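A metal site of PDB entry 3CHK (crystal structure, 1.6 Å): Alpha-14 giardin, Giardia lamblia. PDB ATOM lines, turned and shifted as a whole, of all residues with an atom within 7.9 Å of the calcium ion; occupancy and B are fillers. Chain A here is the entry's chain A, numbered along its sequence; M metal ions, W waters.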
ATOM      1  N   ALA A  61     -20.601  14.942  23.670  1.00  0.00           N
ATOM      2  CA  ALA A  61     -19.737  13.848  23.217  1.00  0.00           C
ATOM      3  C   ALA A  61     -19.789  13.682  21.704  1.00  0.00           C
ATOM      4  O   ALA A  61     -18.757  13.428  21.070  1.00  0.00           O
ATOM      5  CB  ALA A  61     -20.124  12.556  23.913  1.00  0.00           C
ATOM      6  N   PHE A  62     -20.988  13.837  21.144  1.00  0.00           N
ATOM      7  CA  PHE A  62     -21.245  13.724  19.713  1.00  0.00           C
ATOM      8  C   PHE A  62     -20.455  14.790  18.941  1.00  0.00           C
ATOM      9  O   PHE A  62     -19.775  14.471  17.955  1.00  0.00           O
ATOM     10  CB  PHE A  62     -22.747  13.850  19.444  1.00  0.00           C
ATOM     11  CG  PHE A  62     -23.161  13.566  18.019  1.00  0.00           C
ATOM     12  CD1 PHE A  62     -23.221  12.252  17.549  1.00  0.00           C
ATOM     13  CD2 PHE A  62     -23.525  14.601  17.164  1.00  0.00           C
ATOM     14  CE1 PHE A  62     -23.621  11.981  16.225  1.00  0.00           C
ATOM     15  CE2 PHE A  62     -23.933  14.348  15.850  1.00  0.00           C
ATOM     16  CZ  PHE A  62     -23.980  13.037  15.374  1.00  0.00           C
ATOM     17  N   LEU A  63     -20.560  16.045  19.392  1.00  0.00           N
ATOM     18  CA  LEU A  63     -19.830  17.154  18.748  1.00  0.00           C
ATOM     19  C   LEU A  63     -18.331  16.902  18.738  1.00  0.00           C
ATOM     20  O   LEU A  63     -17.679  17.186  17.745  1.00  0.00           O
ATOM     21  CB  LEU A  63     -20.114  18.475  19.458  1.00  0.00           C
ATOM     22  CG  LEU A  63     -21.545  19.024  19.490  1.00  0.00           C
ATOM     23  CD1 LEU A  63     -21.630  20.191  20.495  1.00  0.00           C
ATOM     24  CD2 LEU A  63     -22.012  19.440  18.122  1.00  0.00           C
ATOM     25  N   LYS A  64     -17.821  16.405  19.859  1.00  0.00           N
ATOM     26  CA  LYS A  64     -16.415  16.079  20.033  1.00  0.00           C
ATOM     27  C   LYS A  64     -15.938  15.008  19.036  1.00  0.00           C
ATOM     28  O   LYS A  64     -14.812  15.094  18.549  1.00  0.00           O
ATOM     29  CB  LYS A  64     -16.153  15.603  21.463  1.00  0.00           C
ATOM     30  CG  LYS A  64     -16.035  16.730  22.485  1.00  0.00           C
ATOM     31  CD  LYS A  64     -15.968  16.205  23.905  1.00  0.00           C
ATOM     32  CE  LYS A  64     -15.728  17.340  24.884  1.00  0.00           C
ATOM     33  NZ  LYS A  64     -16.176  17.058  26.294  1.00  0.00           N
ATOM     34  N   LYS A  65     -16.791  14.038  18.727  1.00  0.00           N
ATOM     35  CA  LYS A  65     -16.402  12.984  17.772  1.00  0.00           C
ATOM     36  C   LYS A  65     -16.351  13.473  16.312  1.00  0.00           C
ATOM     37  O   LYS A  65     -15.575  12.936  15.495  1.00  0.00           O
ATOM     38  CB  LYS A  65     -17.272  11.710  17.919  1.00  0.00           C
ATOM     39  CG  LYS A  65     -18.435  11.561  16.925  1.00  0.00           C
ATOM     40  CD  LYS A  65     -19.178  10.210  17.062  1.00  0.00           C
ATOM     41  CE  LYS A  65     -20.213  10.218  18.208  1.00  0.00           C
ATOM     42  NZ  LYS A  65     -20.887   8.894  18.467  1.00  0.00           N
ATOM     43  N   HIS A  66     -17.122  14.504  15.989  1.00  0.00           N
ATOM     44  CA  HIS A  66     -17.249  14.953  14.605  1.00  0.00           C
ATOM     45  C   HIS A  66     -16.508  16.232  14.249  1.00  0.00           C
ATOM     46  O   HIS A  66     -16.209  16.473  13.089  1.00  0.00           O
ATOM     47  CB  HIS A  66     -18.719  15.094  14.228  1.00  0.00           C
ATOM     48  CG  HIS A  66     -19.429  13.787  14.076  1.00  0.00           C
ATOM     49  ND1 HIS A  66     -19.101  12.870  13.098  1.00  0.00           N
ATOM     50  CD2 HIS A  66     -20.451  13.238  14.778  1.00  0.00           C
ATOM     51  CE1 HIS A  66     -19.880  11.809  13.206  1.00  0.00           C
ATOM     52  NE2 HIS A  66     -20.711  12.004  14.218  1.00  0.00           N
ATOM     53  N   LEU A  67     -16.259  17.071  15.248  1.00  0.00           N
ATOM     54  CA  LEU A  67     -15.625  18.362  14.990  1.00  0.00           C
ATOM     55  C   LEU A  67     -14.184  18.347  15.454  1.00  0.00           C
ATOM     56  O   LEU A  67     -13.735  17.406  16.134  1.00  0.00           O
ATOM     57  CB  LEU A  67     -16.405  19.509  15.670  1.00  0.00           C
ATOM     58  CG  LEU A  67     -17.929  19.571  15.455  1.00  0.00           C
ATOM     59  CD1 LEU A  67     -18.533  20.804  16.143  1.00  0.00           C
ATOM     60  CD2 LEU A  67     -18.296  19.590  13.980  1.00  0.00           C
ATOM     61  N   SER A  68     -13.455  19.387  15.050  1.00  0.00           N
ATOM     62  CA  SER A  68     -12.089  19.567  15.491  1.00  0.00           C
ATOM     63  C   SER A  68     -11.712  21.040  15.734  1.00  0.00           C
ATOM     64  O   SER A  68     -12.431  21.961  15.281  1.00  0.00           O
ATOM     65  CB  SER A  68     -11.083  18.928  14.518  1.00  0.00           C
ATOM     66  OG  SER A  68     -11.091  19.589  13.268  1.00  0.00           O
ATOM     67  N   LYS A  69     -10.625  21.190  16.476  1.00  0.00           N
ATOM     68  CA  LYS A  69      -9.852  22.432  16.657  1.00  0.00           C
ATOM     69  C   LYS A  69     -10.743  23.571  17.126  1.00  0.00           C
ATOM     70  O   LYS A  69     -11.651  23.357  17.928  1.00  0.00           O
ATOM     71  CB  LYS A  69      -9.076  22.795  15.381  1.00  0.00           C
ATOM     72  CG  LYS A  69      -8.094  21.692  14.918  1.00  0.00           C
ATOM     73  CD  LYS A  69      -7.725  21.890  13.471  1.00  0.00           C
ATOM     74  CE  LYS A  69      -6.397  21.232  13.126  1.00  0.00           C
ATOM     75  NZ  LYS A  69      -6.045  21.580  11.718  1.00  0.00           N
ATOM     76  N   GLU A  72     -14.697  23.211  16.925  1.00  0.00           N
ATOM     77  CA  GLU A  72     -15.155  22.369  18.057  1.00  0.00           C
ATOM     78  C   GLU A  72     -15.276  23.133  19.382  1.00  0.00           C
ATOM     79  O   GLU A  72     -16.318  23.093  20.047  1.00  0.00           O
ATOM     80  CB  GLU A  72     -14.244  21.167  18.254  1.00  0.00           C
ATOM     81  CG  GLU A  72     -14.690  20.246  19.404  1.00  0.00           C
ATOM     82  CD  GLU A  72     -13.803  19.032  19.564  1.00  0.00           C
ATOM     83  OE1 GLU A  72     -13.484  18.397  18.539  1.00  0.00           O
ATOM     84  OE2 GLU A  72     -13.440  18.674  20.700  1.00  0.00           O
ATOM     85  N   LEU A  76     -18.945  23.773  21.218  1.00  0.00           N
ATOM     86  CA  LEU A  76     -19.178  23.200  22.545  1.00  0.00           C
ATOM     87  C   LEU A  76     -19.650  24.279  23.541  1.00  0.00           C
ATOM     88  O   LEU A  76     -20.542  24.055  24.355  1.00  0.00           O
ATOM     89  CB  LEU A  76     -17.940  22.489  23.060  1.00  0.00           C
ATOM     90  CG  LEU A  76     -17.531  21.175  22.411  1.00  0.00           C
ATOM     91  CD1 LEU A  76     -16.081  20.772  22.833  1.00  0.00           C
ATOM     92  CD2 LEU A  76     -18.581  20.110  22.786  1.00  0.00           C
HETATM   93 CA    CA M   1     -12.823  16.193  17.917  1.00  0.00          CA
HETATM   94  O   HOH W   1     -12.409  14.877  15.722  1.00  0.00           O
HETATM   95  O   HOH W   2     -12.604  16.170  19.991  1.00  0.00           O
HETATM   96  O   HOH W   3     -12.023  13.922  18.907  1.00  0.00           O
HETATM   97  O   HOH W   4     -10.666  17.026  17.367  1.00  0.00           O
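Within 4 Å of the calcium ion: Lys 64, Leu 67 and Glu 72.
The calcium ion is bound by water W2 (2.1 Å), O of Leu 67 (2.3 Å), O of Lys 64 (2.4 Å), water W4 (2.4 Å), OE1 of Glu 72 (2.4 Å), water W1 (2.6 Å) and water W3 (2.6 Å).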
